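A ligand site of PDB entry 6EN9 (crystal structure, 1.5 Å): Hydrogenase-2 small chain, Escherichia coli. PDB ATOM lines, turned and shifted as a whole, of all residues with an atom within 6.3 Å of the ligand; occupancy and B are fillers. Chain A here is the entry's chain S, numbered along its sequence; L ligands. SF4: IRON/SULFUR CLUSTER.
The backbone carbonyl oxygen of Arg 196 lies close to a sulfur (S2) of the ligand. Residues that only touch the ligand: Phe 200, Tyr 221, Gly 227, Pro 228 and Val 248. Hydrophobic or aromatic side chains that line the ligand: His 191, Phe 200, Tyr 221, Pro 228 and Val 248.
SG of Cys 194 is bound to FE4 of the ligand (2.3 Å). S2 of the ligand lies close to N of Arg 197 (3.5 Å). FE1 of the ligand is bound by SG of Cys 219 (2.3 Å). An iron atom (FE3) of the ligand is bound by a ring nitrogen (ND1) of His 191 (2.1 Å). SG of Cys 225 binds FE2 of the ligand (2.3 Å). N of Leu 220 sits close to S3 of the ligand (3.5 Å).
The backbone carbonyl oxygen (O) of His 191 sits at hydrogen-bond distance from the guanidinium group (NH1) of Arg 197. The guanidinium group (NH1) of Arg 196 sits at hydrogen-bond distance from the backbone carbonyl oxygen (O) of Trp 218 (2.9 Å). The side-chain sulfur (SG) of Cys 225 sits close to the backbone NH (N) of Cys 254. N of His 191 lies within hydrogen-bond range of O of Gly 227, 3.1 Å away. NH1 of Arg 197 lies within salt-bridge range of OE1 of Glu 192. SG of Cys 219 sits close to N of Tyr 221. The side-chain sulfur (SG) of Cys 225 lies close to the backbone NH (N) of Gly 227 (3.5 Å). The side-chain sulfur (SG) of Cys 194 sits close to the backbone NH (N) of Arg 196 (3.4 Å).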
ATOM      1  N   ILE A 190      -1.942 -18.063  15.163  1.00  0.00           N
ATOM      2  CA  ILE A 190      -1.298 -19.370  15.217  1.00  0.00           C
ATOM      3  C   ILE A 190      -0.703 -19.623  16.602  1.00  0.00           C
ATOM      4  O   ILE A 190      -0.897 -20.710  17.163  1.00  0.00           O
ATOM      5  CB  ILE A 190      -0.307 -19.539  14.035  1.00  0.00           C
ATOM      6  CG1 ILE A 190      -1.097 -19.631  12.709  1.00  0.00           C
ATOM      7  CG2 ILE A 190       0.570 -20.742  14.247  1.00  0.00           C
ATOM      8  CD1 ILE A 190      -0.240 -19.466  11.448  1.00  0.00           C
ATOM      9  N   HIS A 191       0.008 -18.619  17.135  1.00  0.00           N
ATOM     10  CA  HIS A 191       0.615 -18.766  18.451  1.00  0.00           C
ATOM     11  C   HIS A 191      -0.372 -18.937  19.592  1.00  0.00           C
ATOM     12  O   HIS A 191       0.058 -19.476  20.637  1.00  0.00           O
ATOM     13  CB  HIS A 191       1.475 -17.516  18.690  1.00  0.00           C
ATOM     14  CG  HIS A 191       2.251 -17.459  19.954  1.00  0.00           C
ATOM     15  ND1 HIS A 191       3.424 -18.148  20.177  1.00  0.00           N
ATOM     16  CD2 HIS A 191       2.046 -16.666  21.049  1.00  0.00           C
ATOM     17  CE1 HIS A 191       3.924 -17.769  21.355  1.00  0.00           C
ATOM     18  NE2 HIS A 191       3.088 -16.905  21.917  1.00  0.00           N
ATOM     19  N   GLU A 192      -1.627 -18.579  19.427  1.00  0.00           N
ATOM     20  CA  GLU A 192      -2.651 -18.795  20.422  1.00  0.00           C
ATOM     21  C   GLU A 192      -3.337 -20.143  20.259  1.00  0.00           C
ATOM     22  O   GLU A 192      -4.360 -20.451  20.932  1.00  0.00           O
ATOM     23  CB  GLU A 192      -3.619 -17.642  20.460  1.00  0.00           C
ATOM     24  CG  GLU A 192      -2.967 -16.334  20.929  1.00  0.00           C
ATOM     25  CD  GLU A 192      -2.363 -16.431  22.314  1.00  0.00           C
ATOM     26  OE1 GLU A 192      -1.168 -16.137  22.505  1.00  0.00           O
ATOM     27  OE2 GLU A 192      -3.074 -16.863  23.212  1.00  0.00           O
ATOM     28  N   CYS A 194      -0.894 -23.105  19.243  1.00  0.00           N
ATOM     29  CA  CYS A 194       0.277 -23.805  18.738  1.00  0.00           C
ATOM     30  C   CYS A 194       0.760 -24.800  19.783  1.00  0.00           C
ATOM     31  O   CYS A 194       0.956 -24.450  20.962  1.00  0.00           O
ATOM     32  CB  CYS A 194       1.428 -22.818  18.479  1.00  0.00           C
ATOM     33  SG  CYS A 194       2.923 -23.683  17.910  1.00  0.00           S
ATOM     34  N   GLU A 195       0.995 -26.047  19.360  1.00  0.00           N
ATOM     35  CA  GLU A 195       1.420 -27.111  20.245  1.00  0.00           C
ATOM     36  C   GLU A 195       2.797 -26.911  20.830  1.00  0.00           C
ATOM     37  O   GLU A 195       3.166 -27.660  21.743  1.00  0.00           O
ATOM     38  CB  GLU A 195       1.322 -28.449  19.543  1.00  0.00           C
ATOM     39  CG  GLU A 195       2.290 -28.722  18.402  1.00  0.00           C
ATOM     40  CD  GLU A 195       1.878 -28.207  17.005  1.00  0.00           C
ATOM     41  OE1 GLU A 195       0.962 -27.359  16.873  1.00  0.00           O
ATOM     42  OE2 GLU A 195       2.564 -28.714  16.066  1.00  0.00           O
ATOM     43  N   ARG A 196       3.585 -25.925  20.344  1.00  0.00           N
ATOM     44  CA  ARG A 196       4.892 -25.658  20.919  1.00  0.00           C
ATOM     45  C   ARG A 196       4.825 -24.530  21.899  1.00  0.00           C
ATOM     46  O   ARG A 196       5.864 -24.177  22.477  1.00  0.00           O
ATOM     47  CB  ARG A 196       5.936 -25.370  19.857  1.00  0.00           C
ATOM     48  CG  ARG A 196       6.059 -26.573  18.902  1.00  0.00           C
ATOM     49  CD  ARG A 196       7.189 -26.520  17.957  1.00  0.00           C
ATOM     50  NE  ARG A 196       7.277 -27.747  17.173  1.00  0.00           N
ATOM     51  CZ  ARG A 196       8.335 -28.200  16.549  1.00  0.00           C
ATOM     52  NH1 ARG A 196       9.501 -27.535  16.567  1.00  0.00           N
ATOM     53  NH2 ARG A 196       8.268 -29.350  15.895  1.00  0.00           N
ATOM     54  N   ARG A 197       3.630 -24.030  22.174  1.00  0.00           N
ATOM     55  CA  ARG A 197       3.499 -23.003  23.208  1.00  0.00           C
ATOM     56  C   ARG A 197       4.129 -23.410  24.558  1.00  0.00           C
ATOM     57  O   ARG A 197       4.711 -22.530  25.239  1.00  0.00           O
ATOM     58  CB  ARG A 197       2.059 -22.554  23.379  1.00  0.00           C
ATOM     59  CG  ARG A 197       1.916 -21.424  24.402  1.00  0.00           C
ATOM     60  CD  ARG A 197       2.633 -20.127  24.058  1.00  0.00           C
ATOM     61  NE  ARG A 197       2.162 -19.118  25.008  1.00  0.00           N
ATOM     62  CZ  ARG A 197       1.099 -18.341  24.859  1.00  0.00           C
ATOM     63  NH1 ARG A 197       0.430 -18.259  23.723  1.00  0.00           N
ATOM     64  NH2 ARG A 197       0.701 -17.573  25.864  1.00  0.00           N
ATOM     65  N   PRO A 198       3.977 -24.665  25.007  1.00  0.00           N
ATOM     66  CA  PRO A 198       4.653 -24.986  26.310  1.00  0.00           C
ATOM     67  C   PRO A 198       6.158 -24.711  26.339  1.00  0.00           C
ATOM     68  O   PRO A 198       6.753 -24.339  27.383  1.00  0.00           O
ATOM     69  CB  PRO A 198       4.366 -26.482  26.465  1.00  0.00           C
ATOM     70  CG  PRO A 198       3.090 -26.711  25.662  1.00  0.00           C
ATOM     71  CD  PRO A 198       3.166 -25.781  24.479  1.00  0.00           C
ATOM     72  N   PHE A 200       7.751 -22.451  24.328  1.00  0.00           N
ATOM     73  CA  PHE A 200       7.854 -20.999  24.408  1.00  0.00           C
ATOM     74  C   PHE A 200       7.771 -20.552  25.881  1.00  0.00           C
ATOM     75  O   PHE A 200       8.586 -19.746  26.353  1.00  0.00           O
ATOM     76  CB  PHE A 200       6.740 -20.378  23.580  1.00  0.00           C
ATOM     77  CG  PHE A 200       6.723 -18.880  23.601  1.00  0.00           C
ATOM     78  CD1 PHE A 200       6.025 -18.214  24.561  1.00  0.00           C
ATOM     79  CD2 PHE A 200       7.342 -18.147  22.597  1.00  0.00           C
ATOM     80  CE1 PHE A 200       5.951 -16.830  24.574  1.00  0.00           C
ATOM     81  CE2 PHE A 200       7.263 -16.747  22.609  1.00  0.00           C
ATOM     82  CZ  PHE A 200       6.572 -16.091  23.576  1.00  0.00           C
ATOM     83  N   PHE A 205      13.906 -23.128  23.459  1.00  0.00           N
ATOM     84  CA  PHE A 205      13.979 -22.610  22.104  1.00  0.00           C
ATOM     85  C   PHE A 205      15.052 -23.277  21.278  1.00  0.00           C
ATOM     86  O   PHE A 205      16.183 -23.450  21.704  1.00  0.00           O
ATOM     87  CB  PHE A 205      14.267 -21.108  22.076  1.00  0.00           C
ATOM     88  CG  PHE A 205      13.258 -20.290  22.767  1.00  0.00           C
ATOM     89  CD1 PHE A 205      11.964 -20.123  22.264  1.00  0.00           C
ATOM     90  CD2 PHE A 205      13.582 -19.573  23.922  1.00  0.00           C
ATOM     91  CE1 PHE A 205      11.045 -19.332  22.828  1.00  0.00           C
ATOM     92  CE2 PHE A 205      12.644 -18.773  24.515  1.00  0.00           C
ATOM     93  CZ  PHE A 205      11.357 -18.617  23.991  1.00  0.00           C
ATOM     94  N   TRP A 218      11.354 -28.182  20.002  1.00  0.00           N
ATOM     95  CA  TRP A 218      11.114 -27.037  20.798  1.00  0.00           C
ATOM     96  C   TRP A 218      10.601 -25.865  20.000  1.00  0.00           C
ATOM     97  O   TRP A 218      10.540 -25.913  18.770  1.00  0.00           O
ATOM     98  CB  TRP A 218      12.392 -26.622  21.514  1.00  0.00           C
ATOM     99  CG  TRP A 218      12.804 -27.547  22.648  1.00  0.00           C
ATOM    100  CD1 TRP A 218      12.139 -28.630  23.123  1.00  0.00           C
ATOM    101  CD2 TRP A 218      13.950 -27.370  23.510  1.00  0.00           C
ATOM    102  NE1 TRP A 218      12.859 -29.202  24.177  1.00  0.00           N
ATOM    103  CE2 TRP A 218      13.961 -28.417  24.408  1.00  0.00           C
ATOM    104  CE3 TRP A 218      14.981 -26.427  23.564  1.00  0.00           C
ATOM    105  CZ2 TRP A 218      14.965 -28.557  25.413  1.00  0.00           C
ATOM    106  CZ3 TRP A 218      15.973 -26.570  24.547  1.00  0.00           C
ATOM    107  CH2 TRP A 218      15.953 -27.613  25.439  1.00  0.00           C
ATOM    108  N   CYS A 219      10.246 -24.794  20.693  1.00  0.00           N
ATOM    109  CA  CYS A 219       9.627 -23.640  20.030  1.00  0.00           C
ATOM    110  C   CYS A 219      10.645 -22.985  19.050  1.00  0.00           C
ATOM    111  O   CYS A 219      11.860 -22.933  19.302  1.00  0.00           O
ATOM    112  CB  CYS A 219       9.146 -22.623  21.065  1.00  0.00           C
ATOM    113  SG  CYS A 219       8.660 -20.978  20.485  1.00  0.00           S
ATOM    114  N   LEU A 220      10.073 -22.454  17.921  1.00  0.00           N
ATOM    115  CA  LEU A 220      10.806 -21.815  16.879  1.00  0.00           C
ATOM    116  C   LEU A 220      10.801 -20.285  16.877  1.00  0.00           C
ATOM    117  O   LEU A 220      11.269 -19.657  15.935  1.00  0.00           O
ATOM    118  CB  LEU A 220      10.367 -22.373  15.532  1.00  0.00           C
ATOM    119  CG  LEU A 220      10.306 -23.933  15.470  1.00  0.00           C
ATOM    120  CD1 LEU A 220       9.891 -24.329  14.024  1.00  0.00           C
ATOM    121  CD2 LEU A 220      11.548 -24.603  15.870  1.00  0.00           C
ATOM    122  N   TYR A 221      10.395 -19.693  17.989  1.00  0.00           N
ATOM    123  CA  TYR A 221      10.310 -18.223  18.111  1.00  0.00           C
ATOM    124  C   TYR A 221      11.684 -17.570  17.734  1.00  0.00           C
ATOM    125  O   TYR A 221      11.729 -16.594  16.944  1.00  0.00           O
ATOM    126  CB  TYR A 221       9.893 -17.801  19.564  1.00  0.00           C
ATOM    127  CG  TYR A 221       9.852 -16.305  19.657  1.00  0.00           C
ATOM    128  CD1 TYR A 221       8.851 -15.583  19.036  1.00  0.00           C
ATOM    129  CD2 TYR A 221      10.892 -15.630  20.276  1.00  0.00           C
ATOM    130  CE1 TYR A 221       8.813 -14.213  19.063  1.00  0.00           C
ATOM    131  CE2 TYR A 221      10.901 -14.227  20.281  1.00  0.00           C
ATOM    132  CZ  TYR A 221       9.875 -13.540  19.661  1.00  0.00           C
ATOM    133  OH  TYR A 221       9.897 -12.159  19.639  1.00  0.00           O
ATOM    134  N   HIS A 222      12.761 -18.081  18.316  1.00  0.00           N
ATOM    135  CA  HIS A 222      14.096 -17.491  18.062  1.00  0.00           C
ATOM    136  C   HIS A 222      14.700 -17.845  16.733  1.00  0.00           C
ATOM    137  O   HIS A 222      15.755 -17.312  16.411  1.00  0.00           O
ATOM    138  CB  HIS A 222      15.072 -17.772  19.236  1.00  0.00           C
ATOM    139  CG  HIS A 222      14.787 -16.853  20.382  1.00  0.00           C
ATOM    140  ND1 HIS A 222      15.200 -15.546  20.370  1.00  0.00           N
ATOM    141  CD2 HIS A 222      14.074 -17.013  21.522  1.00  0.00           C
ATOM    142  CE1 HIS A 222      14.744 -14.942  21.460  1.00  0.00           C
ATOM    143  NE2 HIS A 222      14.063 -15.815  22.188  1.00  0.00           N
ATOM    144  N   CYS A 225       9.894 -17.388  14.066  1.00  0.00           N
ATOM    145  CA  CYS A 225       8.497 -17.752  13.906  1.00  0.00           C
ATOM    146  C   CYS A 225       7.557 -16.555  13.978  1.00  0.00           C
ATOM    147  O   CYS A 225       7.543 -15.799  14.976  1.00  0.00           O
ATOM    148  CB  CYS A 225       8.145 -18.838  14.885  1.00  0.00           C
ATOM    149  SG  CYS A 225       6.494 -19.539  14.607  1.00  0.00           S
ATOM    150  N   LYS A 226       6.684 -16.437  12.988  1.00  0.00           N
ATOM    151  CA  LYS A 226       5.720 -15.359  12.924  1.00  0.00           C
ATOM    152  C   LYS A 226       4.367 -15.770  13.432  1.00  0.00           C
ATOM    153  O   LYS A 226       3.386 -14.999  13.361  1.00  0.00           O
ATOM    154  CB  LYS A 226       5.613 -14.841  11.491  1.00  0.00           C
ATOM    155  CG  LYS A 226       6.934 -14.298  10.906  1.00  0.00           C
ATOM    156  CD  LYS A 226       7.699 -13.358  11.838  1.00  0.00           C
ATOM    157  CE  LYS A 226       8.907 -12.783  11.145  1.00  0.00           C
ATOM    158  NZ  LYS A 226       9.852 -13.774  10.611  1.00  0.00           N
ATOM    159  N   GLY A 227       4.255 -16.973  14.034  1.00  0.00           N
ATOM    160  CA  GLY A 227       2.978 -17.377  14.669  1.00  0.00           C
ATOM    161  C   GLY A 227       2.366 -16.343  15.590  1.00  0.00           C
ATOM    162  O   GLY A 227       1.154 -16.163  15.604  1.00  0.00           O
ATOM    163  N   PRO A 228       3.210 -15.612  16.363  1.00  0.00           N
ATOM    164  CA  PRO A 228       2.624 -14.597  17.250  1.00  0.00           C
ATOM    165  C   PRO A 228       1.885 -13.471  16.588  1.00  0.00           C
ATOM    166  O   PRO A 228       1.142 -12.716  17.268  1.00  0.00           O
ATOM    167  CB  PRO A 228       3.824 -14.131  18.063  1.00  0.00           C
ATOM    168  CG  PRO A 228       4.758 -15.285  18.039  1.00  0.00           C
ATOM    169  CD  PRO A 228       4.620 -15.873  16.679  1.00  0.00           C
ATOM    170  N   TRP A 246       2.667 -29.260   9.104  1.00  0.00           N
ATOM    171  CA  TRP A 246       2.640 -27.822   8.895  1.00  0.00           C
ATOM    172  C   TRP A 246       4.075 -27.366   9.079  1.00  0.00           C
ATOM    173  O   TRP A 246       4.927 -28.144   9.518  1.00  0.00           O
ATOM    174  CB  TRP A 246       1.658 -27.089   9.795  1.00  0.00           C
ATOM    175  CG  TRP A 246       1.912 -27.008  11.271  1.00  0.00           C
ATOM    176  CD1 TRP A 246       1.863 -28.015  12.196  1.00  0.00           C
ATOM    177  CD2 TRP A 246       2.141 -25.798  12.007  1.00  0.00           C
ATOM    178  NE1 TRP A 246       2.059 -27.500  13.460  1.00  0.00           N
ATOM    179  CE2 TRP A 246       2.215 -26.138  13.375  1.00  0.00           C
ATOM    180  CE3 TRP A 246       2.252 -24.454  11.646  1.00  0.00           C
ATOM    181  CZ2 TRP A 246       2.407 -25.169  14.370  1.00  0.00           C
ATOM    182  CZ3 TRP A 246       2.452 -23.519  12.615  1.00  0.00           C
ATOM    183  CH2 TRP A 246       2.462 -23.857  13.961  1.00  0.00           C
ATOM    184  N   VAL A 248       5.893 -25.482  11.106  1.00  0.00           N
ATOM    185  CA  VAL A 248       6.536 -25.566  12.448  1.00  0.00           C
ATOM    186  C   VAL A 248       6.721 -27.030  12.828  1.00  0.00           C
ATOM    187  O   VAL A 248       7.759 -27.429  13.328  1.00  0.00           O
ATOM    188  CB  VAL A 248       5.701 -24.811  13.460  1.00  0.00           C
ATOM    189  CG1 VAL A 248       6.081 -25.189  14.879  1.00  0.00           C
ATOM    190  CG2 VAL A 248       5.849 -23.317  13.199  1.00  0.00           C
ATOM    191  N   PRO A 253      10.168 -22.216  11.128  1.00  0.00           N
ATOM    192  CA  PRO A 253       9.231 -21.178  11.611  1.00  0.00           C
ATOM    193  C   PRO A 253       8.125 -20.811  10.624  1.00  0.00           C
ATOM    194  O   PRO A 253       8.324 -20.881   9.417  1.00  0.00           O
ATOM    195  CB  PRO A 253      10.156 -19.952  11.893  1.00  0.00           C
ATOM    196  CG  PRO A 253      11.386 -20.229  11.112  1.00  0.00           C
ATOM    197  CD  PRO A 253      11.558 -21.744  11.106  1.00  0.00           C
ATOM    198  N   CYS A 254       6.987 -20.399  11.157  1.00  0.00           N
ATOM    199  CA  CYS A 254       5.996 -19.658  10.365  1.00  0.00           C
ATOM    200  C   CYS A 254       6.660 -18.394   9.852  1.00  0.00           C
ATOM    201  O   CYS A 254       7.444 -17.762  10.573  1.00  0.00           O
ATOM    202  CB  CYS A 254       4.754 -19.358  11.187  1.00  0.00           C
ATOM    203  SG  CYS A 254       3.559 -18.298  10.373  1.00  0.00           S
HETATM  204 FE1  SF4 L   1       6.743 -20.996  19.248  1.00  0.00          FE
HETATM  205 FE2  SF4 L   1       5.881 -20.205  16.741  1.00  0.00          FE
HETATM  206 FE3  SF4 L   1       4.486 -19.470  18.986  1.00  0.00          FE
HETATM  207 FE4  SF4 L   1       4.440 -22.013  18.143  1.00  0.00          FE
HETATM  208  S1  SF4 L   1       3.598 -20.179  17.009  1.00  0.00           S
HETATM  209  S2  SF4 L   1       4.748 -21.341  20.313  1.00  0.00           S
HETATM  210  S3  SF4 L   1       6.582 -22.302  17.384  1.00  0.00           S
HETATM  211  S4  SF4 L   1       6.593 -18.826  18.431  1.00  0.00           S
